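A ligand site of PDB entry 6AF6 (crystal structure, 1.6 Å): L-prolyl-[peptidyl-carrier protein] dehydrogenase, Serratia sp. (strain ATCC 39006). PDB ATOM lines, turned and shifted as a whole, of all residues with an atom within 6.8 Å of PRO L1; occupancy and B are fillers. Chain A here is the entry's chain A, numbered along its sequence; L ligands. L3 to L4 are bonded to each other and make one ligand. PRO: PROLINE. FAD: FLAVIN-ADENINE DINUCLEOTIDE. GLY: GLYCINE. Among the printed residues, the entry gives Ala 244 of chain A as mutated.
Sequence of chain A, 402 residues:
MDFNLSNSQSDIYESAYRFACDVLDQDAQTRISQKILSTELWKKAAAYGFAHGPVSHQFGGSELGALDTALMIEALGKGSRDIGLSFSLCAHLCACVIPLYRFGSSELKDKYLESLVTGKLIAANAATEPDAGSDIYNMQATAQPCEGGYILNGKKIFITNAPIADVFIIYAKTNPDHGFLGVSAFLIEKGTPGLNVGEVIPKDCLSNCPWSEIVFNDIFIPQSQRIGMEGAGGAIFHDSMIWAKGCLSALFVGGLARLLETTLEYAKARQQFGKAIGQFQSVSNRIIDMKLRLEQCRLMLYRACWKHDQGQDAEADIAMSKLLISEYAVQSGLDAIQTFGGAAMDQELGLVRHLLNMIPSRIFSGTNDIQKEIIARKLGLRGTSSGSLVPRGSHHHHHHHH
N of Ser 365 is in hydrogen-bond range of O of PRO L1 (2.9 Å). The side-chain amide oxygen (OD1) of Asn 125 sits at hydrogen-bond distance from a nitrogen (N) of PRO L1 (3.5 Å). The backbone carbonyl oxygen (O) of Asn 125 lies within hydrogen-bond range of a nitrogen (N3) of FAD L2. The side-chain amide oxygen (OD1) of Asn 125 lies within hydrogen-bond range of a nitrogen (N3) of FAD L2, at 3.3 Å. An oxygen (O2) of FAD L2 lies within hydrogen-bond range of the backbone NH of Thr 128, at 2.8 Å. A nitrogen (N1) of FAD L2 sits at hydrogen-bond distance from the side-chain hydroxyl of Thr 128 (2.9 Å). The backbone NH (N) of Thr 160 is in hydrogen-bond range of an oxygen (O4) of FAD L2. N5 of FAD L2 sits at hydrogen-bond distance from OG1 of Thr 160. The backbone NH (N) of Ala 127 is in hydrogen-bond range of an oxygen (O2) of FAD L2, 2.9 Å away.
O of PRO L1 is in hydrogen-bond range of O2' of FAD L2 (2.7 Å). A nitrogen (N) of PRO L3 is in hydrogen-bond range of an oxygen (O4') of FAD L2.
SD of Met 241 sits close to OXT of PRO L1 (3.6 Å). Merely in contact with PRO L1: Phe 364 and Ala 91. Hydrophobic or aromatic side chains that line PRO L1: Ala 91, Met 241 and Phe 364. Of the 19 residues printed, 5 come within 4 Å of PRO L1. The nearest printed residue that does not touch PRO L1 is Phe 87 (4.1 Å).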
ATOM      1  N   PHE A  87      -1.519  34.026  -3.038  1.00  0.00           N
ATOM      2  CA  PHE A  87      -1.253  32.669  -2.586  1.00  0.00           C
ATOM      3  C   PHE A  87      -2.503  31.800  -2.727  1.00  0.00           C
ATOM      4  O   PHE A  87      -2.427  30.657  -3.150  1.00  0.00           O
ATOM      5  CB  PHE A  87      -0.722  32.683  -1.115  1.00  0.00           C
ATOM      6  CG  PHE A  87      -0.384  31.303  -0.586  1.00  0.00           C
ATOM      7  CD1 PHE A  87       0.814  30.748  -0.903  1.00  0.00           C
ATOM      8  CD2 PHE A  87      -1.289  30.610   0.181  1.00  0.00           C
ATOM      9  CE1 PHE A  87       1.091  29.403  -0.414  1.00  0.00           C
ATOM     10  CE2 PHE A  87      -0.974  29.339   0.677  1.00  0.00           C
ATOM     11  CZ  PHE A  87       0.188  28.767   0.317  1.00  0.00           C
ATOM     12  N   CYS A  90      -2.913  30.848  -6.383  1.00  0.00           N
ATOM     13  CA  CYS A  90      -1.937  29.874  -6.858  1.00  0.00           C
ATOM     14  C   CYS A  90      -2.150  28.518  -6.215  1.00  0.00           C
ATOM     15  O   CYS A  90      -1.863  27.480  -6.838  1.00  0.00           O
ATOM     16  CB  CYS A  90      -0.526  30.431  -6.610  1.00  0.00           C
ATOM     17  SG  CYS A  90      -0.185  31.916  -7.640  1.00  0.00           S
ATOM     18  N   ALA A  91      -2.660  28.463  -4.975  1.00  0.00           N
ATOM     19  CA  ALA A  91      -2.974  27.177  -4.365  1.00  0.00           C
ATOM     20  C   ALA A  91      -4.101  26.499  -5.132  1.00  0.00           C
ATOM     21  O   ALA A  91      -4.041  25.312  -5.447  1.00  0.00           O
ATOM     22  CB  ALA A  91      -3.358  27.356  -2.903  1.00  0.00           C
ATOM     23  N   HIS A  92      -5.128  27.255  -5.484  1.00  0.00           N
ATOM     24  CA  HIS A  92      -6.217  26.708  -6.289  1.00  0.00           C
ATOM     25  C   HIS A  92      -5.707  26.199  -7.624  1.00  0.00           C
ATOM     26  O   HIS A  92      -6.042  25.082  -8.039  1.00  0.00           O
ATOM     27  CB  HIS A  92      -7.243  27.843  -6.440  1.00  0.00           C
ATOM     28  CG  HIS A  92      -8.256  27.645  -7.522  1.00  0.00           C
ATOM     29  ND1 HIS A  92      -9.505  27.097  -7.262  1.00  0.00           N
ATOM     30  CD2 HIS A  92      -8.235  27.951  -8.842  1.00  0.00           C
ATOM     31  CE1 HIS A  92     -10.214  27.082  -8.385  1.00  0.00           C
ATOM     32  NE2 HIS A  92      -9.500  27.651  -9.346  1.00  0.00           N
ATOM     33  N   CYS A  94      -2.456  25.322  -8.480  1.00  0.00           N
ATOM     34  CA  CYS A  94      -1.449  24.259  -8.545  1.00  0.00           C
ATOM     35  C   CYS A  94      -1.898  22.990  -7.886  1.00  0.00           C
ATOM     36  O   CYS A  94      -1.504  21.885  -8.292  1.00  0.00           O
ATOM     37  CB  CYS A  94      -0.123  24.740  -7.893  1.00  0.00           C
ATOM     38  SG  CYS A  94       0.592  26.117  -8.754  1.00  0.00           S
ATOM     39  N   ALA A  95      -2.674  23.081  -6.821  1.00  0.00           N
ATOM     40  CA  ALA A  95      -3.015  21.886  -6.077  1.00  0.00           C
ATOM     41  C   ALA A  95      -4.391  21.375  -6.449  1.00  0.00           C
ATOM     42  O   ALA A  95      -4.780  20.286  -5.959  1.00  0.00           O
ATOM     43  CB  ALA A  95      -2.948  22.159  -4.580  1.00  0.00           C
ATOM     44  N   ASN A 125      -7.311  21.989  -1.561  1.00  0.00           N
ATOM     45  CA  ASN A 125      -6.669  20.674  -1.609  1.00  0.00           C
ATOM     46  C   ASN A 125      -6.452  20.212  -0.178  1.00  0.00           C
ATOM     47  O   ASN A 125      -5.942  20.970   0.652  1.00  0.00           O
ATOM     48  CB  ASN A 125      -5.355  20.789  -2.399  1.00  0.00           C
ATOM     49  CG  ASN A 125      -4.228  19.946  -1.828  1.00  0.00           C
ATOM     50  OD1 ASN A 125      -3.412  20.398  -1.036  1.00  0.00           O
ATOM     51  ND2 ASN A 125      -4.154  18.748  -2.268  1.00  0.00           N
ATOM     52  N   ALA A 127      -4.825  17.395   2.045  1.00  0.00           N
ATOM     53  CA  ALA A 127      -3.967  16.232   2.216  1.00  0.00           C
ATOM     54  C   ALA A 127      -3.467  16.114   3.652  1.00  0.00           C
ATOM     55  O   ALA A 127      -3.566  15.035   4.271  1.00  0.00           O
ATOM     56  CB  ALA A 127      -2.777  16.318   1.240  1.00  0.00           C
ATOM     57  N   THR A 128      -2.916  17.221   4.192  1.00  0.00           N
ATOM     58  CA  THR A 128      -2.346  17.204   5.533  1.00  0.00           C
ATOM     59  C   THR A 128      -3.332  16.813   6.606  1.00  0.00           C
ATOM     60  O   THR A 128      -4.494  17.241   6.626  1.00  0.00           O
ATOM     61  CB  THR A 128      -1.756  18.602   5.819  1.00  0.00           C
ATOM     62  OG1 THR A 128      -0.818  18.826   4.799  1.00  0.00           O
ATOM     63  CG2 THR A 128      -1.101  18.641   7.219  1.00  0.00           C
ATOM     64  N   PHE A 158      -4.989  22.578   8.118  1.00  0.00           N
ATOM     65  CA  PHE A 158      -4.138  23.573   7.415  1.00  0.00           C
ATOM     66  C   PHE A 158      -4.576  23.754   5.961  1.00  0.00           C
ATOM     67  O   PHE A 158      -3.761  23.936   5.044  1.00  0.00           O
ATOM     68  CB  PHE A 158      -2.629  23.179   7.448  1.00  0.00           C
ATOM     69  CG  PHE A 158      -2.072  23.012   8.823  1.00  0.00           C
ATOM     70  CD1 PHE A 158      -2.590  23.654   9.946  1.00  0.00           C
ATOM     71  CD2 PHE A 158      -0.978  22.155   8.991  1.00  0.00           C
ATOM     72  CE1 PHE A 158      -1.987  23.499  11.206  1.00  0.00           C
ATOM     73  CE2 PHE A 158      -0.401  22.026  10.297  1.00  0.00           C
ATOM     74  CZ  PHE A 158      -0.890  22.677  11.330  1.00  0.00           C
ATOM     75  N   THR A 160      -5.728  25.501   2.931  1.00  0.00           N
ATOM     76  CA  THR A 160      -5.860  26.815   2.256  1.00  0.00           C
ATOM     77  C   THR A 160      -7.168  26.838   1.463  1.00  0.00           C
ATOM     78  O   THR A 160      -7.489  25.867   0.758  1.00  0.00           O
ATOM     79  CB  THR A 160      -4.653  26.992   1.363  1.00  0.00           C
ATOM     80  OG1 THR A 160      -3.514  27.079   2.249  1.00  0.00           O
ATOM     81  CG2 THR A 160      -4.781  28.321   0.574  1.00  0.00           C
ATOM     82  N   PHE A 237      -0.721  13.500  -5.852  1.00  0.00           N
ATOM     83  CA  PHE A 237      -0.317  14.514  -4.871  1.00  0.00           C
ATOM     84  C   PHE A 237       1.105  14.960  -5.163  1.00  0.00           C
ATOM     85  O   PHE A 237       1.430  16.175  -5.123  1.00  0.00           O
ATOM     86  CB  PHE A 237      -0.407  13.957  -3.457  1.00  0.00           C
ATOM     87  CG  PHE A 237       0.008  14.949  -2.384  1.00  0.00           C
ATOM     88  CD1 PHE A 237      -0.842  16.007  -2.067  1.00  0.00           C
ATOM     89  CD2 PHE A 237       1.236  14.855  -1.753  1.00  0.00           C
ATOM     90  CE1 PHE A 237      -0.474  16.966  -1.115  1.00  0.00           C
ATOM     91  CE2 PHE A 237       1.608  15.815  -0.782  1.00  0.00           C
ATOM     92  CZ  PHE A 237       0.735  16.838  -0.467  1.00  0.00           C
ATOM     93  N   MET A 241       2.470  18.717  -6.075  1.00  0.00           N
ATOM     94  CA  MET A 241       3.435  19.495  -5.268  1.00  0.00           C
ATOM     95  C   MET A 241       4.596  19.970  -6.098  1.00  0.00           C
ATOM     96  O   MET A 241       5.200  21.002  -5.750  1.00  0.00           O
ATOM     97  CB  MET A 241       3.954  18.694  -4.047  1.00  0.00           C
ATOM     98  CG  MET A 241       2.882  18.503  -2.948  1.00  0.00           C
ATOM     99  SD  MET A 241       2.074  20.049  -2.313  1.00  0.00           S
ATOM    100  CE  MET A 241       0.427  20.095  -3.113  1.00  0.00           C
ATOM    101  N   ALA A 244       3.175  23.202  -7.389  1.00  0.00           N
ATOM    102  CA  ALA A 244       3.143  24.113  -6.251  1.00  0.00           C
ATOM    103  C   ALA A 244       4.535  24.608  -5.881  1.00  0.00           C
ATOM    104  O   ALA A 244       4.736  25.825  -5.659  1.00  0.00           O
ATOM    105  CB  ALA A 244       2.448  23.442  -5.071  1.00  0.00           C
ATOM    106  N   LEU A 248       4.317  28.027  -7.993  1.00  0.00           N
ATOM    107  CA  LEU A 248       3.824  28.905  -6.942  1.00  0.00           C
ATOM    108  C   LEU A 248       4.963  29.689  -6.298  1.00  0.00           C
ATOM    109  O   LEU A 248       4.811  30.879  -6.015  1.00  0.00           O
ATOM    110  CB  LEU A 248       3.043  28.103  -5.909  1.00  0.00           C
ATOM    111  CG  LEU A 248       2.238  28.875  -4.884  1.00  0.00           C
ATOM    112  CD1 LEU A 248       1.102  27.971  -4.411  1.00  0.00           C
ATOM    113  CD2 LEU A 248       3.095  29.258  -3.666  1.00  0.00           C
ATOM    114  N   ILE A 363       7.648  26.313   4.653  1.00  0.00           N
ATOM    115  CA  ILE A 363       6.846  25.222   5.237  1.00  0.00           C
ATOM    116  C   ILE A 363       5.910  24.594   4.208  1.00  0.00           C
ATOM    117  O   ILE A 363       5.810  23.359   4.087  1.00  0.00           O
ATOM    118  CB  ILE A 363       6.052  25.740   6.432  1.00  0.00           C
ATOM    119  CG1 ILE A 363       6.983  26.363   7.494  1.00  0.00           C
ATOM    120  CG2 ILE A 363       5.185  24.636   7.083  1.00  0.00           C
ATOM    121  CD1 ILE A 363       6.230  27.201   8.503  1.00  0.00           C
ATOM    122  N   PHE A 364       5.206  25.419   3.418  1.00  0.00           N
ATOM    123  CA  PHE A 364       4.196  24.696   2.669  1.00  0.00           C
ATOM    124  C   PHE A 364       4.804  24.018   1.415  1.00  0.00           C
ATOM    125  O   PHE A 364       5.967  24.223   1.003  1.00  0.00           O
ATOM    126  CB  PHE A 364       2.991  25.576   2.339  1.00  0.00           C
ATOM    127  CG  PHE A 364       3.353  26.922   1.807  1.00  0.00           C
ATOM    128  CD1 PHE A 364       4.036  27.036   0.627  1.00  0.00           C
ATOM    129  CD2 PHE A 364       3.015  28.058   2.486  1.00  0.00           C
ATOM    130  CE1 PHE A 364       4.399  28.270   0.133  1.00  0.00           C
ATOM    131  CE2 PHE A 364       3.360  29.322   2.015  1.00  0.00           C
ATOM    132  CZ  PHE A 364       4.041  29.435   0.825  1.00  0.00           C
ATOM    133  N   SER A 365       4.012  23.058   0.919  1.00  0.00           N
ATOM    134  CA  SER A 365       4.411  22.127  -0.126  1.00  0.00           C
ATOM    135  C   SER A 365       5.620  21.285   0.261  1.00  0.00           C
ATOM    136  O   SER A 365       6.296  20.742  -0.627  1.00  0.00           O
ATOM    137  CB  SER A 365       4.634  22.801  -1.456  1.00  0.00           C
ATOM    138  OG  SER A 365       5.828  23.571  -1.471  1.00  0.00           O
ATOM    139  N   GLY A 366       5.877  21.172   1.557  1.00  0.00           N
ATOM    140  CA  GLY A 366       6.972  20.348   2.041  1.00  0.00           C
ATOM    141  C   GLY A 366       7.983  21.267   2.674  1.00  0.00           C
ATOM    142  O   GLY A 366       8.409  22.239   2.040  1.00  0.00           O
HETATM  143  N   PRO L   1      -1.203  23.104  -0.867  1.00  0.00           N
HETATM  144  CA  PRO L   1       0.219  22.899  -0.581  1.00  0.00           C
HETATM  145  C   PRO L   1       0.552  21.938   0.579  1.00  0.00           C
HETATM  146  O   PRO L   1       1.320  22.212   1.496  1.00  0.00           O
HETATM  147  CB  PRO L   1       0.693  24.320  -0.322  1.00  0.00           C
HETATM  148  CG  PRO L   1      -0.045  25.097  -1.460  1.00  0.00           C
HETATM  149  CD  PRO L   1      -1.420  24.406  -1.522  1.00  0.00           C
HETATM  150  OXT PRO L   1       0.075  20.797   0.569  1.00  0.00           O
HETATM  151  PA  FAD L   2       5.963  18.581  10.642  1.00  0.00           P
HETATM  152  O1A FAD L   2       5.511  18.298  11.976  1.00  0.00           O
HETATM  153  O2A FAD L   2       5.989  17.557   9.667  1.00  0.00           O
HETATM  154  O5B FAD L   2       7.469  19.168  10.722  1.00  0.00           O
HETATM  155  C5B FAD L   2       7.959  19.725  11.961  1.00  0.00           C
HETATM  156  C4B FAD L   2       9.483  19.914  11.807  1.00  0.00           C
HETATM  157  O4B FAD L   2      10.075  18.603  11.668  1.00  0.00           O
HETATM  158  C3B FAD L   2       9.905  20.683  10.550  1.00  0.00           C
HETATM  159  O3B FAD L   2      11.130  21.377  10.821  1.00  0.00           O
HETATM  160  C2B FAD L   2      10.180  19.546   9.566  1.00  0.00           C
HETATM  161  O2B FAD L   2      11.092  19.906   8.554  1.00  0.00           O
HETATM  162  C1B FAD L   2      10.857  18.551  10.517  1.00  0.00           C
HETATM  163  N9A FAD L   2      10.891  17.186  10.005  1.00  0.00           N
HETATM  164  C8A FAD L   2       9.818  16.327   9.813  1.00  0.00           C
HETATM  165  N7A FAD L   2      10.170  15.184   9.265  1.00  0.00           N
HETATM  166  C5A FAD L   2      11.529  15.328   9.018  1.00  0.00           C
HETATM  167  C6A FAD L   2      12.490  14.480   8.414  1.00  0.00           C
HETATM  168  N6A FAD L   2      12.207  13.265   7.943  1.00  0.00           N
HETATM  169  N1A FAD L   2      13.777  14.935   8.338  1.00  0.00           N
HETATM  170  C2A FAD L   2      14.055  16.146   8.841  1.00  0.00           C
HETATM  171  N3A FAD L   2      13.242  17.020   9.440  1.00  0.00           N
HETATM  172  C4A FAD L   2      11.984  16.541   9.491  1.00  0.00           C
HETATM  173  N1  FAD L   2      -1.699  21.250   3.522  1.00  0.00           N
HETATM  174  C2  FAD L   2      -2.707  20.782   2.714  1.00  0.00           C
HETATM  175  O2  FAD L   2      -3.030  19.584   2.652  1.00  0.00           O
HETATM  176  N3  FAD L   2      -3.424  21.661   1.975  1.00  0.00           N
HETATM  177  C4  FAD L   2      -3.194  23.054   1.932  1.00  0.00           C
HETATM  178  O4  FAD L   2      -3.919  23.808   1.266  1.00  0.00           O
HETATM  179  C4X FAD L   2      -2.097  23.517   2.762  1.00  0.00           C
HETATM  180  N5  FAD L   2      -1.821  24.805   2.756  1.00  0.00           N
HETATM  181  C5X FAD L   2      -0.866  25.268   3.628  1.00  0.00           C
HETATM  182  C6  FAD L   2      -0.583  26.629   3.637  1.00  0.00           C
HETATM  183  C7  FAD L   2       0.401  27.131   4.479  1.00  0.00           C
HETATM  184  C7M FAD L   2       0.672  28.622   4.472  1.00  0.00           C
HETATM  185  C8  FAD L   2       1.163  26.264   5.258  1.00  0.00           C
HETATM  186  C8M FAD L   2       2.244  26.802   6.199  1.00  0.00           C
HETATM  187  C9  FAD L   2       0.872  24.906   5.261  1.00  0.00           C
HETATM  188  C9A FAD L   2      -0.086  24.394   4.403  1.00  0.00           C
HETATM  189  N10 FAD L   2      -0.370  23.003   4.335  1.00  0.00           N
HETATM  190  C10 FAD L   2      -1.423  22.544   3.557  1.00  0.00           C
HETATM  191  C1' FAD L   2       0.314  22.067   5.270  1.00  0.00           C
HETATM  192  C2' FAD L   2       1.785  21.781   4.934  1.00  0.00           C
HETATM  193  O2' FAD L   2       1.798  20.882   3.840  1.00  0.00           O
HETATM  194  C3' FAD L   2       2.464  21.176   6.177  1.00  0.00           C
HETATM  195  O3' FAD L   2       2.488  22.234   7.128  1.00  0.00           O
HETATM  196  C4' FAD L   2       3.876  20.702   5.877  1.00  0.00           C
HETATM  197  O4' FAD L   2       3.857  19.588   4.990  1.00  0.00           O
HETATM  198  C5' FAD L   2       4.671  20.422   7.133  1.00  0.00           C
HETATM  199  O5' FAD L   2       3.909  19.541   8.023  1.00  0.00           O
HETATM  200  P   FAD L   2       3.664  19.875   9.475  1.00  0.00           P
HETATM  201  O1P FAD L   2       3.169  21.305   9.625  1.00  0.00           O
HETATM  202  O2P FAD L   2       2.886  18.788  10.064  1.00  0.00           O
HETATM  203  O3P FAD L   2       5.202  19.871  10.091  1.00  0.00           O
HETATM  204  N   PRO L   3       3.121  17.324   3.254  1.00  0.00           N
HETATM  205  CA  PRO L   3       3.595  17.193   1.890  1.00  0.00           C
HETATM  206  C   PRO L   3       5.060  16.780   1.688  1.00  0.00           C
HETATM  207  O   PRO L   3       5.773  16.386   2.631  1.00  0.00           O
HETATM  208  CB  PRO L   3       3.268  18.573   1.307  1.00  0.00           C
HETATM  209  CG  PRO L   3       1.878  18.808   1.916  1.00  0.00           C
HETATM  210  CD  PRO L   3       1.811  18.012   3.269  1.00  0.00           C
HETATM  211  N   GLY L   4       5.473  16.788   0.421  1.00  0.00           N
HETATM  212  CA  GLY L   4       6.609  16.010  -0.032  1.00  0.00           C
HETATM  213  C   GLY L   4       6.340  15.597  -1.484  1.00  0.00           C
HETATM  214  O   GLY L   4       6.498  16.402  -2.407  1.00  0.00           O
HETATM  215  OXT GLY L   4       5.929  14.469  -1.778  1.00  0.00           O
